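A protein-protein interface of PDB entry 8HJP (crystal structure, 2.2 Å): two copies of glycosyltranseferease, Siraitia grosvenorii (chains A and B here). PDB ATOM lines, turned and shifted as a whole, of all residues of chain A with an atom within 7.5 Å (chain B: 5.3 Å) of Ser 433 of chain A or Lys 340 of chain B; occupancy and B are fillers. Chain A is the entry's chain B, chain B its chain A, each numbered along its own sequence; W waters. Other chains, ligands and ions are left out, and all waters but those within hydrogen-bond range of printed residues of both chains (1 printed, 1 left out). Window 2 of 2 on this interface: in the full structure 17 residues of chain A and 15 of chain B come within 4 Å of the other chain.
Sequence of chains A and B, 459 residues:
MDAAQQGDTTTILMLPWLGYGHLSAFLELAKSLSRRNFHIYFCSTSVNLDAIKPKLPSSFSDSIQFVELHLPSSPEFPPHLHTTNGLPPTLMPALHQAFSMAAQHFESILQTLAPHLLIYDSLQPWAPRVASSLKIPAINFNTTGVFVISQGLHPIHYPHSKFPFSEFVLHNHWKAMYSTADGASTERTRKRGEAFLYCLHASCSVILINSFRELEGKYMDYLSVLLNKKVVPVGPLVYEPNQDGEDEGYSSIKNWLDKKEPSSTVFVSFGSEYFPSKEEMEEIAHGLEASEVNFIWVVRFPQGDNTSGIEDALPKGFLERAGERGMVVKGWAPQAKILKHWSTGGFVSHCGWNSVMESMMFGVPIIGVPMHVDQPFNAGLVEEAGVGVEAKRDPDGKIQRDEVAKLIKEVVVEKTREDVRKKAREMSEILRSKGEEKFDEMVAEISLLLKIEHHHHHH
OE2 of Glu 240 of chain B is in hydrogen-bond range of OG of Ser 433 of chain A, at 3.3 Å.
NE1 of Trp 342 of chain B sits at hydrogen-bond distance from OE1 of Glu 429 of chain A (3.3 Å).
The side-chain hydroxyl (OG) of Ser 433 of chain A is in hydrogen-bond range of the guanidinium group (NH2) of Arg 432 of chain B (3.2 Å).
NZ of Lys 340 of chain B is in salt-bridge range of OE2 of Glu 240 of chain B, at 2.7 Å.
The side-chain carboxylate (OE1) of Glu 240 of chain B is in salt-bridge range of the guanidinium group (NH1) of Arg 432 of chain B (2.8 Å).
OG of Ser 433 of chain A sits at hydrogen-bond distance from O of Glu 429 of chain A, at 3.1 Å.
Glu 426 of chain A touches Trp 342 of chain B.
Ser 433 of chain A touches Lys 340 of chain B (OG to NZ, 3.9 Å).
Ser 433 of chain A touches just these residues of chain B: Glu 240 (3.3 Å), Lys 340 (3.9 Å) and Arg 432 (3.2 Å).
Of the printed residues of chain A, Lys 340 of chain B touches Ser 433 (3.9 Å).
Of the printed residues of chain A, Arg 432 of chain B touches Ser 433.
Of the printed residues of chain A, Glu 240 of chain B touches Ser 433 (3.3 Å).
Of the printed residues of chain B, Glu 426 of chain A touches Trp 342 (3.4 Å).
The nearest printed residue of chain B that does not touch Ser 433 of chain A is Phe 362 of chain B (6.4 Å).
The nearest residue of chain A that does not touch Lys 340 of chain B is Glu 429 of chain A (6.0 Å).
The nearest printed residue of chain B that does not touch Glu 429 of chain A is Arg 432 of chain B (5.4 Å).
Hydrophobic or aromatic side chains of chain B that line the printed part of chain A: Trp 342.
Along chain B the printed residues that touch a printed residue of chain A span positions 240 to 432.
Of the 13 printed residues of chain A, 3 touch a printed residue of chain B.
Printed residues of chain A that touch a printed residue of chain B: Glu 426, Glu 429 and Ser 433.
Among the printed residues, 5 pairs touch across the chains.
Position printed for both chains: 432.
Of the 5 pairs that touch across the chains among the printed residues, none has its exchanged pair printed and touching as well.
Water W1 lies within hydrogen-bond range of NE of Arg 432 of chain B (3.0 Å), O of Glu 429 of chain A (3.1 Å) and OG of Ser 433 of chain A (3.1 Å).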
ATOM      1  N   MET A 361     -33.303 -17.093   5.975  1.00  0.00           N
ATOM      2  CA  MET A 361     -32.183 -16.792   5.089  1.00  0.00           C
ATOM      3  C   MET A 361     -30.874 -17.337   5.646  1.00  0.00           C
ATOM      4  O   MET A 361     -30.044 -17.863   4.896  1.00  0.00           O
ATOM      5  CB  MET A 361     -32.081 -15.281   4.872  1.00  0.00           C
ATOM      6  CG  MET A 361     -30.939 -14.843   3.958  1.00  0.00           C
ATOM      7  SD  MET A 361     -31.107 -15.347   2.237  1.00  0.00           S
ATOM      8  CE  MET A 361     -32.363 -14.203   1.671  1.00  0.00           C
ATOM      9  N   GLU A 426     -32.193 -26.529   4.051  1.00  0.00           N
ATOM     10  CA  GLU A 426     -32.706 -26.549   2.687  1.00  0.00           C
ATOM     11  C   GLU A 426     -33.312 -25.201   2.331  1.00  0.00           C
ATOM     12  O   GLU A 426     -33.065 -24.668   1.241  1.00  0.00           O
ATOM     13  CB  GLU A 426     -33.749 -27.658   2.527  1.00  0.00           C
ATOM     14  CG  GLU A 426     -33.181 -29.064   2.492  1.00  0.00           C
ATOM     15  CD  GLU A 426     -34.259 -30.134   2.534  1.00  0.00           C
ATOM     16  OE1 GLU A 426     -35.452 -29.781   2.633  1.00  0.00           O
ATOM     17  OE2 GLU A 426     -33.910 -31.330   2.469  1.00  0.00           O
ATOM     18  N   MET A 427     -34.086 -24.622   3.253  1.00  0.00           N
ATOM     19  CA  MET A 427     -34.738 -23.344   2.991  1.00  0.00           C
ATOM     20  C   MET A 427     -33.718 -22.230   2.792  1.00  0.00           C
ATOM     21  O   MET A 427     -33.858 -21.409   1.878  1.00  0.00           O
ATOM     22  CB  MET A 427     -35.683 -23.003   4.144  1.00  0.00           C
ATOM     23  CG  MET A 427     -36.436 -21.694   3.983  1.00  0.00           C
ATOM     24  SD  MET A 427     -37.554 -21.659   2.574  1.00  0.00           S
ATOM     25  CE  MET A 427     -38.813 -22.805   3.129  1.00  0.00           C
ATOM     26  N   SER A 428     -32.687 -22.182   3.643  1.00  0.00           N
ATOM     27  CA  SER A 428     -31.628 -21.192   3.462  1.00  0.00           C
ATOM     28  C   SER A 428     -30.957 -21.364   2.107  1.00  0.00           C
ATOM     29  O   SER A 428     -30.666 -20.382   1.416  1.00  0.00           O
ATOM     30  CB  SER A 428     -30.598 -21.291   4.587  1.00  0.00           C
ATOM     31  OG  SER A 428     -29.539 -20.370   4.385  1.00  0.00           O
ATOM     32  N   GLU A 429     -30.720 -22.613   1.701  1.00  0.00           N
ATOM     33  CA  GLU A 429     -30.133 -22.869   0.389  1.00  0.00           C
ATOM     34  C   GLU A 429     -31.040 -22.352  -0.719  1.00  0.00           C
ATOM     35  O   GLU A 429     -30.561 -21.779  -1.704  1.00  0.00           O
ATOM     36  CB  GLU A 429     -29.851 -24.363   0.213  1.00  0.00           C
ATOM     37  CG  GLU A 429     -28.647 -24.866   1.005  1.00  0.00           C
ATOM     38  CD  GLU A 429     -28.404 -26.353   0.827  1.00  0.00           C
ATOM     39  OE1 GLU A 429     -29.287 -27.034   0.268  1.00  0.00           O
ATOM     40  OE2 GLU A 429     -27.330 -26.841   1.242  1.00  0.00           O
ATOM     41  N   ILE A 430     -32.354 -22.563  -0.590  1.00  0.00           N
ATOM     42  CA  ILE A 430     -33.288 -22.024  -1.576  1.00  0.00           C
ATOM     43  C   ILE A 430     -33.170 -20.504  -1.635  1.00  0.00           C
ATOM     44  O   ILE A 430     -33.070 -19.910  -2.715  1.00  0.00           O
ATOM     45  CB  ILE A 430     -34.728 -22.454  -1.247  1.00  0.00           C
ATOM     46  CG1 ILE A 430     -34.894 -23.969  -1.380  1.00  0.00           C
ATOM     47  CG2 ILE A 430     -35.723 -21.708  -2.120  1.00  0.00           C
ATOM     48  CD1 ILE A 430     -36.270 -24.461  -0.981  1.00  0.00           C
ATOM     49  N   LEU A 431     -33.166 -19.857  -0.467  1.00  0.00           N
ATOM     50  CA  LEU A 431     -33.186 -18.396  -0.411  1.00  0.00           C
ATOM     51  C   LEU A 431     -31.867 -17.809  -0.898  1.00  0.00           C
ATOM     52  O   LEU A 431     -31.855 -16.820  -1.641  1.00  0.00           O
ATOM     53  CB  LEU A 431     -33.514 -17.942   1.011  1.00  0.00           C
ATOM     54  CG  LEU A 431     -34.980 -18.207   1.358  1.00  0.00           C
ATOM     55  CD1 LEU A 431     -35.311 -17.836   2.798  1.00  0.00           C
ATOM     56  CD2 LEU A 431     -35.872 -17.456   0.381  1.00  0.00           C
ATOM     57  N   ARG A 432     -30.749 -18.404  -0.481  1.00  0.00           N
ATOM     58  CA  ARG A 432     -29.434 -17.931  -0.898  1.00  0.00           C
ATOM     59  C   ARG A 432     -29.238 -18.096  -2.399  1.00  0.00           C
ATOM     60  O   ARG A 432     -28.534 -17.297  -3.026  1.00  0.00           O
ATOM     61  CB  ARG A 432     -28.337 -18.666  -0.127  1.00  0.00           C
ATOM     62  CG  ARG A 432     -28.276 -18.263   1.321  1.00  0.00           C
ATOM     63  CD  ARG A 432     -27.961 -16.789   1.425  1.00  0.00           C
ATOM     64  NE  ARG A 432     -27.274 -16.448   2.664  1.00  0.00           N
ATOM     65  CZ  ARG A 432     -27.038 -15.201   3.056  1.00  0.00           C
ATOM     66  NH1 ARG A 432     -27.434 -14.180   2.305  1.00  0.00           N
ATOM     67  NH2 ARG A 432     -26.413 -14.974   4.201  1.00  0.00           N
ATOM     68  N   SER A 433     -29.839 -19.138  -2.984  1.00  0.00           N
ATOM     69  CA  SER A 433     -29.725 -19.383  -4.417  1.00  0.00           C
ATOM     70  C   SER A 433     -30.412 -18.320  -5.266  1.00  0.00           C
ATOM     71  O   SER A 433     -30.081 -18.189  -6.451  1.00  0.00           O
ATOM     72  CB  SER A 433     -30.379 -20.730  -4.747  1.00  0.00           C
ATOM     73  OG  SER A 433     -29.509 -21.830  -4.586  1.00  0.00           O
ATOM     74  N   LYS A 434     -31.353 -17.571  -4.700  1.00  0.00           N
ATOM     75  CA  LYS A 434     -32.083 -16.582  -5.480  1.00  0.00           C
ATOM     76  C   LYS A 434     -31.200 -15.394  -5.867  1.00  0.00           C
ATOM     77  O   LYS A 434     -30.355 -14.936  -5.088  1.00  0.00           O
ATOM     78  CB  LYS A 434     -33.308 -16.116  -4.701  1.00  0.00           C
ATOM     79  CG  LYS A 434     -34.168 -17.301  -4.280  1.00  0.00           C
ATOM     80  CD  LYS A 434     -34.719 -18.030  -5.496  1.00  0.00           C
ATOM     81  CE  LYS A 434     -35.628 -19.186  -5.099  1.00  0.00           C
ATOM     82  NZ  LYS A 434     -36.472 -19.663  -6.235  1.00  0.00           N
ATOM     83  N   GLY A 435     -31.399 -14.895  -7.086  1.00  0.00           N
ATOM     84  CA  GLY A 435     -30.564 -13.832  -7.614  1.00  0.00           C
ATOM     85  C   GLY A 435     -31.366 -12.607  -8.000  1.00  0.00           C
ATOM     86  O   GLY A 435     -32.428 -12.348  -7.425  1.00  0.00           O
ATOM     87  N   GLU A 436     -30.875 -11.852  -8.983  1.00  0.00           N
ATOM     88  CA  GLU A 436     -31.489 -10.580  -9.344  1.00  0.00           C
ATOM     89  C   GLU A 436     -32.850 -10.748 -10.013  1.00  0.00           C
ATOM     90  O   GLU A 436     -33.589  -9.762 -10.128  1.00  0.00           O
ATOM     91  CB  GLU A 436     -30.521  -9.779 -10.215  1.00  0.00           C
ATOM     92  CG  GLU A 436     -29.166  -9.605  -9.524  1.00  0.00           C
ATOM     93  CD  GLU A 436     -28.273  -8.558 -10.161  1.00  0.00           C
ATOM     94  OE1 GLU A 436     -28.571  -8.106 -11.286  1.00  0.00           O
ATOM     95  OE2 GLU A 436     -27.263  -8.187  -9.524  1.00  0.00           O
ATOM     96  N   GLU A 437     -33.202 -11.964 -10.445  1.00  0.00           N
ATOM     97  CA  GLU A 437     -34.498 -12.203 -11.075  1.00  0.00           C
ATOM     98  C   GLU A 437     -35.638 -11.858 -10.133  1.00  0.00           C
ATOM     99  O   GLU A 437     -36.771 -11.656 -10.582  1.00  0.00           O
ATOM    100  CB  GLU A 437     -34.609 -13.665 -11.508  1.00  0.00           C
ATOM    101  CG  GLU A 437     -34.807 -14.619 -10.340  1.00  0.00           C
ATOM    102  CD  GLU A 437     -33.501 -15.140  -9.779  1.00  0.00           C
ATOM    103  OE1 GLU A 437     -32.430 -14.712 -10.260  1.00  0.00           O
ATOM    104  OE2 GLU A 437     -33.543 -15.972  -8.847  1.00  0.00           O
ATOM    105  N   GLU B 240     -26.975 -20.133 -12.298  1.00  0.00           N
ATOM    106  CA  GLU B 240     -27.780 -20.936 -11.390  1.00  0.00           C
ATOM    107  C   GLU B 240     -28.847 -21.673 -12.182  1.00  0.00           C
ATOM    108  O   GLU B 240     -29.704 -21.023 -12.803  1.00  0.00           O
ATOM    109  CB  GLU B 240     -28.422 -20.056 -10.324  1.00  0.00           C
ATOM    110  CG  GLU B 240     -28.887 -20.809  -9.091  1.00  0.00           C
ATOM    111  CD  GLU B 240     -27.763 -21.090  -8.111  1.00  0.00           C
ATOM    112  OE1 GLU B 240     -26.830 -20.266  -8.018  1.00  0.00           O
ATOM    113  OE2 GLU B 240     -27.816 -22.132  -7.427  1.00  0.00           O
ATOM    114  N   PRO B 241     -28.834 -23.004 -12.199  1.00  0.00           N
ATOM    115  CA  PRO B 241     -29.789 -23.755 -13.022  1.00  0.00           C
ATOM    116  C   PRO B 241     -31.214 -23.702 -12.488  1.00  0.00           C
ATOM    117  O   PRO B 241     -31.470 -23.415 -11.318  1.00  0.00           O
ATOM    118  CB  PRO B 241     -29.231 -25.178 -12.974  1.00  0.00           C
ATOM    119  CG  PRO B 241     -28.597 -25.253 -11.621  1.00  0.00           C
ATOM    120  CD  PRO B 241     -27.944 -23.902 -11.441  1.00  0.00           C
ATOM    121  N   GLN B 335     -23.638 -29.921 -15.357  1.00  0.00           N
ATOM    122  CA  GLN B 335     -22.575 -29.812 -14.363  1.00  0.00           C
ATOM    123  C   GLN B 335     -23.042 -29.079 -13.112  1.00  0.00           C
ATOM    124  O   GLN B 335     -22.826 -29.550 -11.989  1.00  0.00           O
ATOM    125  CB  GLN B 335     -21.363 -29.114 -14.974  1.00  0.00           C
ATOM    126  CG  GLN B 335     -20.368 -28.612 -13.948  1.00  0.00           C
ATOM    127  CD  GLN B 335     -19.021 -28.289 -14.559  1.00  0.00           C
ATOM    128  OE1 GLN B 335     -18.555 -28.983 -15.461  1.00  0.00           O
ATOM    129  NE2 GLN B 335     -18.390 -27.228 -14.071  1.00  0.00           N
ATOM    130  N   ALA B 336     -23.678 -27.917 -13.284  1.00  0.00           N
ATOM    131  CA  ALA B 336     -24.109 -27.145 -12.122  1.00  0.00           C
ATOM    132  C   ALA B 336     -25.111 -27.925 -11.281  1.00  0.00           C
ATOM    133  O   ALA B 336     -25.056 -27.888 -10.046  1.00  0.00           O
ATOM    134  CB  ALA B 336     -24.703 -25.809 -12.567  1.00  0.00           C
ATOM    135  N   LYS B 337     -26.040 -28.631 -11.933  1.00  0.00           N
ATOM    136  CA  LYS B 337     -27.047 -29.381 -11.190  1.00  0.00           C
ATOM    137  C   LYS B 337     -26.408 -30.512 -10.391  1.00  0.00           C
ATOM    138  O   LYS B 337     -26.788 -30.761  -9.240  1.00  0.00           O
ATOM    139  CB  LYS B 337     -28.116 -29.913 -12.144  1.00  0.00           C
ATOM    140  CG  LYS B 337     -28.908 -28.809 -12.823  1.00  0.00           C
ATOM    141  CD  LYS B 337     -29.781 -29.340 -13.942  1.00  0.00           C
ATOM    142  CE  LYS B 337     -31.099 -28.584 -13.996  1.00  0.00           C
ATOM    143  NZ  LYS B 337     -31.972 -29.041 -15.113  1.00  0.00           N
ATOM    144  N   ILE B 338     -25.446 -31.216 -10.992  1.00  0.00           N
ATOM    145  CA  ILE B 338     -24.775 -32.310 -10.298  1.00  0.00           C
ATOM    146  C   ILE B 338     -23.969 -31.785  -9.115  1.00  0.00           C
ATOM    147  O   ILE B 338     -23.963 -32.388  -8.035  1.00  0.00           O
ATOM    148  CB  ILE B 338     -23.896 -33.102 -11.283  1.00  0.00           C
ATOM    149  CG1 ILE B 338     -24.770 -33.741 -12.366  1.00  0.00           C
ATOM    150  CG2 ILE B 338     -23.080 -34.159 -10.550  1.00  0.00           C
ATOM    151  CD1 ILE B 338     -24.000 -34.283 -13.546  1.00  0.00           C
ATOM    152  N   LEU B 339     -23.280 -30.655  -9.294  1.00  0.00           N
ATOM    153  CA  LEU B 339     -22.490 -30.092  -8.203  1.00  0.00           C
ATOM    154  C   LEU B 339     -23.368 -29.696  -7.023  1.00  0.00           C
ATOM    155  O   LEU B 339     -22.938 -29.792  -5.866  1.00  0.00           O
ATOM    156  CB  LEU B 339     -21.687 -28.887  -8.704  1.00  0.00           C
ATOM    157  CG  LEU B 339     -20.502 -29.172  -9.636  1.00  0.00           C
ATOM    158  CD1 LEU B 339     -19.795 -27.884 -10.041  1.00  0.00           C
ATOM    159  CD2 LEU B 339     -19.521 -30.135  -8.984  1.00  0.00           C
ATOM    160  N   LYS B 340     -24.592 -29.238  -7.291  1.00  0.00           N
ATOM    161  CA  LYS B 340     -25.522 -28.851  -6.236  1.00  0.00           C
ATOM    162  C   LYS B 340     -26.145 -30.037  -5.501  1.00  0.00           C
ATOM    163  O   LYS B 340     -26.638 -29.852  -4.381  1.00  0.00           O
ATOM    164  CB  LYS B 340     -26.599 -27.932  -6.821  1.00  0.00           C
ATOM    165  CG  LYS B 340     -26.008 -26.599  -7.266  1.00  0.00           C
ATOM    166  CD  LYS B 340     -27.032 -25.632  -7.831  1.00  0.00           C
ATOM    167  CE  LYS B 340     -28.068 -25.233  -6.797  1.00  0.00           C
ATOM    168  NZ  LYS B 340     -29.157 -24.435  -7.428  1.00  0.00           N
ATOM    169  N   HIS B 341     -26.168 -31.229  -6.103  1.00  0.00           N
ATOM    170  CA  HIS B 341     -26.764 -32.388  -5.444  1.00  0.00           C
ATOM    171  C   HIS B 341     -26.000 -32.727  -4.166  1.00  0.00           C
ATOM    172  O   HIS B 341     -24.771 -32.644  -4.118  1.00  0.00           O
ATOM    173  CB  HIS B 341     -26.783 -33.591  -6.392  1.00  0.00           C
ATOM    174  CG  HIS B 341     -27.806 -34.627  -6.039  1.00  0.00           C
ATOM    175  ND1 HIS B 341     -27.801 -35.300  -4.835  1.00  0.00           N
ATOM    176  CD2 HIS B 341     -28.866 -35.105  -6.731  1.00  0.00           C
ATOM    177  CE1 HIS B 341     -28.812 -36.148  -4.803  1.00  0.00           C
ATOM    178  NE2 HIS B 341     -29.475 -36.050  -5.941  1.00  0.00           N
ATOM    179  N   TRP B 342     -26.741 -33.109  -3.119  1.00  0.00           N
ATOM    180  CA  TRP B 342     -26.120 -33.469  -1.845  1.00  0.00           C
ATOM    181  C   TRP B 342     -25.257 -34.729  -1.904  1.00  0.00           C
ATOM    182  O   TRP B 342     -24.389 -34.897  -1.044  1.00  0.00           O
ATOM    183  CB  TRP B 342     -27.174 -33.619  -0.749  1.00  0.00           C
ATOM    184  CG  TRP B 342     -27.703 -32.304  -0.222  1.00  0.00           C
ATOM    185  CD1 TRP B 342     -27.335 -31.054  -0.620  1.00  0.00           C
ATOM    186  CD2 TRP B 342     -28.662 -32.116   0.836  1.00  0.00           C
ATOM    187  NE1 TRP B 342     -28.012 -30.101   0.102  1.00  0.00           N
ATOM    188  CE2 TRP B 342     -28.831 -30.726   1.003  1.00  0.00           C
ATOM    189  CE3 TRP B 342     -29.398 -32.987   1.648  1.00  0.00           C
ATOM    190  CZ2 TRP B 342     -29.708 -30.187   1.945  1.00  0.00           C
ATOM    191  CZ3 TRP B 342     -30.263 -32.450   2.583  1.00  0.00           C
ATOM    192  CH2 TRP B 342     -30.410 -31.065   2.726  1.00  0.00           C
ATOM    193  N   PHE B 362     -20.881 -23.480  -4.893  1.00  0.00           N
ATOM    194  CA  PHE B 362     -21.685 -24.587  -4.389  1.00  0.00           C
ATOM    195  C   PHE B 362     -21.007 -25.363  -3.265  1.00  0.00           C
ATOM    196  O   PHE B 362     -21.589 -26.333  -2.768  1.00  0.00           O
ATOM    197  CB  PHE B 362     -22.029 -25.555  -5.527  1.00  0.00           C
ATOM    198  CG  PHE B 362     -22.646 -24.895  -6.727  1.00  0.00           C
ATOM    199  CD1 PHE B 362     -23.579 -23.882  -6.580  1.00  0.00           C
ATOM    200  CD2 PHE B 362     -22.299 -25.299  -8.007  1.00  0.00           C
ATOM    201  CE1 PHE B 362     -24.146 -23.278  -7.687  1.00  0.00           C
ATOM    202  CE2 PHE B 362     -22.862 -24.701  -9.116  1.00  0.00           C
ATOM    203  CZ  PHE B 362     -23.788 -23.689  -8.957  1.00  0.00           C
ATOM    204  N   ARG B 432     -22.366 -17.011  -1.505  1.00  0.00           N
ATOM    205  CA  ARG B 432     -23.821 -16.909  -1.464  1.00  0.00           C
ATOM    206  C   ARG B 432     -24.267 -15.580  -0.859  1.00  0.00           C
ATOM    207  O   ARG B 432     -25.324 -15.053  -1.234  1.00  0.00           O
ATOM    208  CB  ARG B 432     -24.416 -18.099  -0.693  1.00  0.00           C
ATOM    209  CG  ARG B 432     -24.376 -19.418  -1.461  1.00  0.00           C
ATOM    210  CD  ARG B 432     -24.948 -19.304  -2.874  1.00  0.00           C
ATOM    211  NE  ARG B 432     -25.350 -20.606  -3.412  1.00  0.00           N
ATOM    212  CZ  ARG B 432     -25.957 -20.775  -4.584  1.00  0.00           C
ATOM    213  NH1 ARG B 432     -26.228 -19.728  -5.355  1.00  0.00           N
ATOM    214  NH2 ARG B 432     -26.296 -21.990  -4.989  1.00  0.00           N
HETATM  215  O   HOH W   1     -27.559 -22.149  -2.164  1.00  0.00           O
